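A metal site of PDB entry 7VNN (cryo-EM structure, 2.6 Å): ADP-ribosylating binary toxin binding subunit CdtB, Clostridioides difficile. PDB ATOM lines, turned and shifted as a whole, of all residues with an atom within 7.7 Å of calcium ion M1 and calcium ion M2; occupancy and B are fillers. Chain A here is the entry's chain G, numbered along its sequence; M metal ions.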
ATOM      1  N   LEU A  18       8.994  10.260 -19.848  1.00  0.00           N
ATOM      2  CA  LEU A  18       8.257  11.287 -20.587  1.00  0.00           C
ATOM      3  C   LEU A  18       7.146  10.654 -21.416  1.00  0.00           C
ATOM      4  O   LEU A  18       7.364   9.668 -22.128  1.00  0.00           O
ATOM      5  CB  LEU A  18       9.217  12.062 -21.497  1.00  0.00           C
ATOM      6  CG  LEU A  18       8.583  12.825 -22.656  1.00  0.00           C
ATOM      7  CD1 LEU A  18       7.792  14.014 -22.147  1.00  0.00           C
ATOM      8  CD2 LEU A  18       9.636  13.267 -23.657  1.00  0.00           C
ATOM      9  N   ASP A  19       5.950  11.243 -21.317  1.00  0.00           N
ATOM     10  CA  ASP A  19       4.764  10.730 -22.022  1.00  0.00           C
ATOM     11  C   ASP A  19       4.088  11.915 -22.699  1.00  0.00           C
ATOM     12  O   ASP A  19       3.315  12.650 -22.070  1.00  0.00           O
ATOM     13  CB  ASP A  19       3.829  10.022 -21.050  1.00  0.00           C
ATOM     14  CG  ASP A  19       2.999   8.959 -21.717  1.00  0.00           C
ATOM     15  OD1 ASP A  19       2.991   8.900 -22.970  1.00  0.00           O
ATOM     16  OD2 ASP A  19       2.341   8.169 -21.004  1.00  0.00           O
ATOM     17  N   THR A  20       4.371  12.091 -23.995  1.00  0.00           N
ATOM     18  CA  THR A  20       3.835  13.235 -24.720  1.00  0.00           C
ATOM     19  C   THR A  20       2.336  13.105 -25.000  1.00  0.00           C
ATOM     20  O   THR A  20       1.583  14.064 -24.800  1.00  0.00           O
ATOM     21  CB  THR A  20       4.594  13.425 -26.028  1.00  0.00           C
ATOM     22  OG1 THR A  20       5.999  13.465 -25.768  1.00  0.00           O
ATOM     23  CG2 THR A  20       4.182  14.720 -26.715  1.00  0.00           C
ATOM     24  N   ASP A  21       1.895  11.941 -25.461  1.00  0.00           N
ATOM     25  CA  ASP A  21       0.498  11.727 -25.820  1.00  0.00           C
ATOM     26  C   ASP A  21      -0.342  11.167 -24.689  1.00  0.00           C
ATOM     27  O   ASP A  21      -1.553  10.989 -24.863  1.00  0.00           O
ATOM     28  CB  ASP A  21       0.399  10.820 -27.053  1.00  0.00           C
ATOM     29  CG  ASP A  21       1.166   9.522 -26.875  1.00  0.00           C
ATOM     30  OD1 ASP A  21       1.822   9.354 -25.834  1.00  0.00           O
ATOM     31  OD2 ASP A  21       1.119   8.677 -27.792  1.00  0.00           O
ATOM     32  N   ASN A  22       0.262  10.887 -23.528  1.00  0.00           N
ATOM     33  CA  ASN A  22      -0.458  10.428 -22.348  1.00  0.00           C
ATOM     34  C   ASN A  22      -1.262   9.161 -22.635  1.00  0.00           C
ATOM     35  O   ASN A  22      -2.474   9.103 -22.445  1.00  0.00           O
ATOM     36  CB  ASN A  22      -1.366  11.521 -21.795  1.00  0.00           C
ATOM     37  CG  ASN A  22      -0.699  12.882 -21.790  1.00  0.00           C
ATOM     38  OD1 ASN A  22      -1.287  13.876 -22.214  1.00  0.00           O
ATOM     39  ND2 ASN A  22       0.533  12.939 -21.292  1.00  0.00           N
ATOM     40  N   ASP A  23      -0.569   8.121 -23.109  1.00  0.00           N
ATOM     41  CA  ASP A  23      -1.195   6.830 -23.372  1.00  0.00           C
ATOM     42  C   ASP A  23      -0.573   5.715 -22.539  1.00  0.00           C
ATOM     43  O   ASP A  23      -0.665   4.540 -22.921  1.00  0.00           O
ATOM     44  CB  ASP A  23      -1.137   6.492 -24.854  1.00  0.00           C
ATOM     45  CG  ASP A  23       0.283   6.256 -25.346  1.00  0.00           C
ATOM     46  OD1 ASP A  23       1.237   6.718 -24.699  1.00  0.00           O
ATOM     47  OD2 ASP A  23       0.433   5.598 -26.400  1.00  0.00           O
ATOM     48  N   ASN A  24       0.058   6.061 -21.414  1.00  0.00           N
ATOM     49  CA  ASN A  24       0.668   5.139 -20.460  1.00  0.00           C
ATOM     50  C   ASN A  24       1.897   4.422 -21.002  1.00  0.00           C
ATOM     51  O   ASN A  24       2.287   3.382 -20.457  1.00  0.00           O
ATOM     52  CB  ASN A  24      -0.328   4.085 -19.954  1.00  0.00           C
ATOM     53  CG  ASN A  24      -1.600   4.695 -19.413  1.00  0.00           C
ATOM     54  OD1 ASN A  24      -1.585   5.410 -18.413  1.00  0.00           O
ATOM     55  ND2 ASN A  24      -2.715   4.408 -20.079  1.00  0.00           N
ATOM     56  N   ILE A  25       2.513   4.926 -22.070  1.00  0.00           N
ATOM     57  CA  ILE A  25       3.741   4.348 -22.601  1.00  0.00           C
ATOM     58  C   ILE A  25       4.732   5.478 -22.817  1.00  0.00           C
ATOM     59  O   ILE A  25       4.406   6.472 -23.479  1.00  0.00           O
ATOM     60  CB  ILE A  25       3.512   3.567 -23.901  1.00  0.00           C
ATOM     61  CG1 ILE A  25       2.428   2.513 -23.720  1.00  0.00           C
ATOM     62  CG2 ILE A  25       4.790   2.855 -24.294  1.00  0.00           C
ATOM     63  CD1 ILE A  25       1.957   1.906 -25.024  1.00  0.00           C
ATOM     64  N   PRO A  26       5.952   5.385 -22.288  1.00  0.00           N
ATOM     65  CA  PRO A  26       6.939   6.454 -22.502  1.00  0.00           C
ATOM     66  C   PRO A  26       7.308   6.591 -23.979  1.00  0.00           C
ATOM     67  O   PRO A  26       7.214   5.636 -24.755  1.00  0.00           O
ATOM     68  CB  PRO A  26       8.141   5.998 -21.668  1.00  0.00           C
ATOM     69  CG  PRO A  26       7.548   5.136 -20.621  1.00  0.00           C
ATOM     70  CD  PRO A  26       6.405   4.423 -21.278  1.00  0.00           C
ATOM     71  N   ASP A  27       7.723   7.802 -24.358  1.00  0.00           N
ATOM     72  CA  ASP A  27       8.092   8.060 -25.747  1.00  0.00           C
ATOM     73  C   ASP A  27       9.297   7.236 -26.169  1.00  0.00           C
ATOM     74  O   ASP A  27       9.356   6.752 -27.301  1.00  0.00           O
ATOM     75  CB  ASP A  27       8.354   9.550 -25.960  1.00  0.00           C
ATOM     76  CG  ASP A  27       7.142  10.408 -25.712  1.00  0.00           C
ATOM     77  OD1 ASP A  27       6.009   9.918 -25.919  1.00  0.00           O
ATOM     78  OD2 ASP A  27       7.298  11.586 -25.331  1.00  0.00           O
ATOM     79  N   SER A  28      10.275   7.074 -25.281  1.00  0.00           N
ATOM     80  CA  SER A  28      11.455   6.275 -25.609  1.00  0.00           C
ATOM     81  C   SER A  28      11.070   4.807 -25.825  1.00  0.00           C
ATOM     82  O   SER A  28      11.618   4.149 -26.722  1.00  0.00           O
ATOM     83  CB  SER A  28      12.502   6.403 -24.514  1.00  0.00           C
ATOM     84  OG  SER A  28      11.946   6.161 -23.234  1.00  0.00           O
ATOM     85  N   TYR A  29      10.147   4.295 -25.015  1.00  0.00           N
ATOM     86  CA  TYR A  29       9.707   2.906 -25.175  1.00  0.00           C
ATOM     87  C   TYR A  29       9.081   2.678 -26.546  1.00  0.00           C
ATOM     88  O   TYR A  29       9.380   1.690 -27.217  1.00  0.00           O
ATOM     89  CB  TYR A  29       8.724   2.520 -24.078  1.00  0.00           C
ATOM     90  CG  TYR A  29       9.313   2.352 -22.688  1.00  0.00           C
ATOM     91  CD1 TYR A  29      10.520   2.931 -22.333  1.00  0.00           C
ATOM     92  CD2 TYR A  29       8.636   1.622 -21.721  1.00  0.00           C
ATOM     93  CE1 TYR A  29      11.044   2.781 -21.061  1.00  0.00           C
ATOM     94  CE2 TYR A  29       9.147   1.465 -20.450  1.00  0.00           C
ATOM     95  CZ  TYR A  29      10.348   2.043 -20.130  1.00  0.00           C
ATOM     96  OH  TYR A  29      10.860   1.886 -18.859  1.00  0.00           O
ATOM     97  N   GLU A  30       8.190   3.585 -26.966  1.00  0.00           N
ATOM     98  CA  GLU A  30       7.559   3.430 -28.267  1.00  0.00           C
ATOM     99  C   GLU A  30       8.551   3.649 -29.399  1.00  0.00           C
ATOM    100  O   GLU A  30       8.443   3.025 -30.454  1.00  0.00           O
ATOM    101  CB  GLU A  30       6.371   4.381 -28.396  1.00  0.00           C
ATOM    102  CG  GLU A  30       5.214   4.025 -27.492  1.00  0.00           C
ATOM    103  CD  GLU A  30       4.040   4.951 -27.637  1.00  0.00           C
ATOM    104  OE1 GLU A  30       4.153   5.955 -28.361  1.00  0.00           O
ATOM    105  OE2 GLU A  30       2.993   4.674 -27.027  1.00  0.00           O
ATOM    106  N   TYR A  34       8.869  -2.111 -26.927  1.00  0.00           N
ATOM    107  CA  TYR A  34       8.332  -2.415 -25.609  1.00  0.00           C
ATOM    108  C   TYR A  34       7.436  -3.649 -25.694  1.00  0.00           C
ATOM    109  O   TYR A  34       7.152  -4.166 -26.780  1.00  0.00           O
ATOM    110  CB  TYR A  34       7.553  -1.236 -25.037  1.00  0.00           C
ATOM    111  CG  TYR A  34       6.335  -0.838 -25.847  1.00  0.00           C
ATOM    112  CD1 TYR A  34       6.445   0.009 -26.931  1.00  0.00           C
ATOM    113  CD2 TYR A  34       5.079  -1.331 -25.521  1.00  0.00           C
ATOM    114  CE1 TYR A  34       5.341   0.363 -27.668  1.00  0.00           C
ATOM    115  CE2 TYR A  34       3.969  -0.981 -26.251  1.00  0.00           C
ATOM    116  CZ  TYR A  34       4.103  -0.132 -27.328  1.00  0.00           C
ATOM    117  OH  TYR A  34       2.998   0.222 -28.065  1.00  0.00           O
ATOM    118  N   SER A  58       5.401   2.025 -31.894  1.00  0.00           N
ATOM    119  CA  SER A  58       4.213   2.818 -32.219  1.00  0.00           C
ATOM    120  C   SER A  58       4.582   4.297 -32.243  1.00  0.00           C
ATOM    121  O   SER A  58       5.704   4.688 -31.916  1.00  0.00           O
ATOM    122  CB  SER A  58       3.093   2.546 -31.218  1.00  0.00           C
ATOM    123  OG  SER A  58       3.435   2.996 -29.917  1.00  0.00           O
ATOM    124  N   ASN A  59       3.602   5.105 -32.655  1.00  0.00           N
ATOM    125  CA  ASN A  59       3.786   6.540 -32.765  1.00  0.00           C
ATOM    126  C   ASN A  59       3.797   7.184 -31.388  1.00  0.00           C
ATOM    127  O   ASN A  59       2.855   7.013 -30.608  1.00  0.00           O
ATOM    128  CB  ASN A  59       2.676   7.134 -33.625  1.00  0.00           C
ATOM    129  CG  ASN A  59       2.977   8.543 -34.100  1.00  0.00           C
ATOM    130  OD1 ASN A  59       3.848   9.210 -33.563  1.00  0.00           O
ATOM    131  ND2 ASN A  59       2.234   8.994 -35.104  1.00  0.00           N
ATOM    132  N   TYR A  60       4.856   7.935 -31.074  1.00  0.00           N
ATOM    133  CA  TYR A  60       4.985   8.550 -29.758  1.00  0.00           C
ATOM    134  C   TYR A  60       4.309   9.914 -29.670  1.00  0.00           C
ATOM    135  O   TYR A  60       4.196  10.449 -28.555  1.00  0.00           O
ATOM    136  CB  TYR A  60       6.462   8.655 -29.352  1.00  0.00           C
ATOM    137  CG  TYR A  60       7.216   9.817 -29.945  1.00  0.00           C
ATOM    138  CD1 TYR A  60       7.785   9.728 -31.209  1.00  0.00           C
ATOM    139  CD2 TYR A  60       7.385  10.997 -29.231  1.00  0.00           C
ATOM    140  CE1 TYR A  60       8.486  10.785 -31.753  1.00  0.00           C
ATOM    141  CE2 TYR A  60       8.080  12.062 -29.774  1.00  0.00           C
ATOM    142  CZ  TYR A  60       8.630  11.949 -31.025  1.00  0.00           C
ATOM    143  OH  TYR A  60       9.325  13.001 -31.562  1.00  0.00           O
ATOM    144  N   LEU A  61       3.863  10.481 -30.782  1.00  0.00           N
ATOM    145  CA  LEU A  61       3.089  11.711 -30.774  1.00  0.00           C
ATOM    146  C   LEU A  61       1.606  11.480 -30.984  1.00  0.00           C
ATOM    147  O   LEU A  61       0.832  12.445 -30.989  1.00  0.00           O
ATOM    148  CB  LEU A  61       3.615  12.674 -31.833  1.00  0.00           C
ATOM    149  CG  LEU A  61       4.967  13.347 -31.573  1.00  0.00           C
ATOM    150  CD1 LEU A  61       5.280  14.340 -32.684  1.00  0.00           C
ATOM    151  CD2 LEU A  61       4.980  14.030 -30.228  1.00  0.00           C
ATOM    152  N   GLU A  62       1.176  10.227 -31.154  1.00  0.00           N
ATOM    153  CA  GLU A  62      -0.208   9.886 -31.431  1.00  0.00           C
ATOM    154  C   GLU A  62      -0.666   8.788 -30.497  1.00  0.00           C
ATOM    155  O   GLU A  62       0.053   7.807 -30.272  1.00  0.00           O
ATOM    156  CB  GLU A  62      -0.384   9.443 -32.889  1.00  0.00           C
ATOM    157  CG  GLU A  62      -1.818   9.523 -33.395  1.00  0.00           C
ATOM    158  CD  GLU A  62      -2.243  10.942 -33.710  1.00  0.00           C
ATOM    159  OE1 GLU A  62      -1.624  11.571 -34.584  1.00  0.00           O
ATOM    160  OE2 GLU A  62      -3.210  11.421 -33.070  1.00  0.00           O
ATOM    161  N   SER A  63      -1.870   8.947 -29.935  1.00  0.00           N
ATOM    162  CA  SER A  63      -2.395   7.949 -29.013  1.00  0.00           C
ATOM    163  C   SER A  63      -3.051   6.774 -29.742  1.00  0.00           C
ATOM    164  O   SER A  63      -3.117   5.673 -29.196  1.00  0.00           O
ATOM    165  CB  SER A  63      -3.401   8.601 -28.068  1.00  0.00           C
ATOM    166  OG  SER A  63      -3.758   7.715 -27.019  1.00  0.00           O
ATOM    167  N   ASN A  64      -3.538   7.000 -30.965  1.00  0.00           N
ATOM    168  CA  ASN A  64      -4.155   5.960 -31.783  1.00  0.00           C
ATOM    169  C   ASN A  64      -3.366   5.876 -33.085  1.00  0.00           C
ATOM    170  O   ASN A  64      -3.703   6.543 -34.070  1.00  0.00           O
ATOM    171  CB  ASN A  64      -5.636   6.270 -32.029  1.00  0.00           C
ATOM    172  CG  ASN A  64      -6.489   6.009 -30.817  1.00  0.00           C
ATOM    173  OD1 ASN A  64      -6.444   6.743 -29.838  1.00  0.00           O
ATOM    174  ND2 ASN A  64      -7.300   4.964 -30.888  1.00  0.00           N
ATOM    175  N   THR A  65      -2.315   5.053 -33.086  1.00  0.00           N
ATOM    176  CA  THR A  65      -1.448   4.957 -34.255  1.00  0.00           C
ATOM    177  C   THR A  65      -2.195   4.410 -35.458  1.00  0.00           C
ATOM    178  O   THR A  65      -2.038   4.915 -36.577  1.00  0.00           O
ATOM    179  CB  THR A  65      -0.238   4.084 -33.930  1.00  0.00           C
ATOM    180  OG1 THR A  65       0.516   4.682 -32.865  1.00  0.00           O
ATOM    181  CG2 THR A  65       0.658   3.939 -35.145  1.00  0.00           C
ATOM    182  N   THR A  71      -6.546   2.713 -28.146  1.00  0.00           N
ATOM    183  CA  THR A  71      -5.262   3.370 -28.041  1.00  0.00           C
ATOM    184  C   THR A  71      -4.132   2.355 -28.236  1.00  0.00           C
ATOM    185  O   THR A  71      -4.349   1.177 -28.496  1.00  0.00           O
ATOM    186  CB  THR A  71      -5.126   4.069 -26.697  1.00  0.00           C
ATOM    187  OG1 THR A  71      -4.754   3.118 -25.692  1.00  0.00           O
ATOM    188  CG2 THR A  71      -6.431   4.730 -26.301  1.00  0.00           C
ATOM    189  N   ASP A  72      -2.897   2.843 -28.116  1.00  0.00           N
ATOM    190  CA  ASP A  72      -1.736   1.967 -28.230  1.00  0.00           C
ATOM    191  C   ASP A  72      -1.644   1.021 -27.043  1.00  0.00           C
ATOM    192  O   ASP A  72      -1.374  -0.180 -27.212  1.00  0.00           O
ATOM    193  CB  ASP A  72      -0.461   2.791 -28.353  1.00  0.00           C
ATOM    194  CG  ASP A  72      -0.400   3.581 -29.647  1.00  0.00           C
ATOM    195  OD1 ASP A  72      -1.175   3.261 -30.576  1.00  0.00           O
ATOM    196  OD2 ASP A  72       0.411   4.523 -29.740  1.00  0.00           O
ATOM    197  N   TYR A  73      -1.861   1.533 -25.829  1.00  0.00           N
ATOM    198  CA  TYR A  73      -1.772   0.690 -24.641  1.00  0.00           C
ATOM    199  C   TYR A  73      -2.897  -0.330 -24.592  1.00  0.00           C
ATOM    200  O   TYR A  73      -2.675  -1.480 -24.203  1.00  0.00           O
ATOM    201  CB  TYR A  73      -1.780   1.554 -23.381  1.00  0.00           C
ATOM    202  CG  TYR A  73      -1.792   0.737 -22.105  1.00  0.00           C
ATOM    203  CD1 TYR A  73      -0.649   0.072 -21.684  1.00  0.00           C
ATOM    204  CD2 TYR A  73      -2.944   0.618 -21.346  1.00  0.00           C
ATOM    205  CE1 TYR A  73      -0.657  -0.675 -20.522  1.00  0.00           C
ATOM    206  CE2 TYR A  73      -2.952  -0.129 -20.184  1.00  0.00           C
ATOM    207  CZ  TYR A  73      -1.808  -0.769 -19.775  1.00  0.00           C
ATOM    208  OH  TYR A  73      -1.817  -1.514 -18.628  1.00  0.00           O
ATOM    209  N   PRO A  91       0.155  -2.104 -32.336  1.00  0.00           N
ATOM    210  CA  PRO A  91      -0.455  -0.814 -32.687  1.00  0.00           C
ATOM    211  C   PRO A  91      -0.454  -0.510 -34.167  1.00  0.00           C
ATOM    212  O   PRO A  91      -1.165   0.412 -34.595  1.00  0.00           O
ATOM    213  CB  PRO A  91       0.409   0.201 -31.917  1.00  0.00           C
ATOM    214  CG  PRO A  91       0.987  -0.591 -30.796  1.00  0.00           C
ATOM    215  CD  PRO A  91       1.247  -1.949 -31.360  1.00  0.00           C
HETATM  216 CA    CA M   1       3.379   7.581 -25.399  1.00  0.00          CA
HETATM  217 CA    CA M   2       1.404   6.430 -28.682  1.00  0.00          CA
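Six residues have an atom within 4 Å of calcium ion M2: Asp 21, Asp 23, Glu 30, Asn 59, Glu 62 and Asp 72. The nearest printed residue that does not touch calcium ion M2 is Ser 63 (4.1 Å).
Merely in contact with calcium ion M1: Asp 27 (3.6 Å). Six residues have an atom within 4 Å of calcium ion M1: Asp 19, Asp 21, Asp 23, Ile 25, Asp 27 and Glu 30.
The side-chain amide oxygen (OD1) of Asn 59 is in hydrogen-bond range of the backbone NH (N) of Leu 61 (3.1 Å). O of Leu 18 lies within hydrogen-bond range of N of Asp 27, 2.9 Å away. The side-chain amide nitrogen (ND2) of Asn 22 lies within hydrogen-bond range of the backbone carbonyl oxygen (O) of Asp 19 (2.9 Å). The side-chain carboxylate of Asp 72 lies within hydrogen-bond range of the side-chain hydroxyl of Thr 65. OE1 of Glu 30 lies close to N of Tyr 60, 3.4 Å away. The side-chain carboxylate (OD2) of Asp 72 lies close to the side-chain hydroxyl (OG) of Ser 58 (3.4 Å). The backbone carbonyl oxygen (O) of Ser 63 is in hydrogen-bond range of the backbone NH (N) of Asp 72 (3.0 Å). OG of Ser 58 sits close to OE2 of Glu 30 (3.4 Å).
The side-chain carboxylate (OD1) of Asp 21 is bound to calcium ion M1 (2.4 Å). The side-chain carboxylate (OD1) of Asp 23 is bound to calcium ion M1 (2.4 Å). O of Ile 25 is bound to calcium ion M1 (2.4 Å). OD1 of Asp 19 binds calcium ion M1, at 2.8 Å.
Calcium ion M2 is bound by the side-chain carboxylate (OD2) of Asp 72 (2.4 Å), the side-chain carboxylate (OD2) of Asp 21 (2.4 Å), the backbone carbonyl oxygen (O) of Asn 59 (2.5 Å), the backbone carbonyl oxygen (O) of Glu 62 (2.5 Å), the side-chain carboxylate (OD2) of Asp 23 (2.6 Å), the side-chain carboxylate (OE1) of Glu 30 (2.8 Å) and the side-chain carboxylate (OE2) of Glu 30 (2.9 Å).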
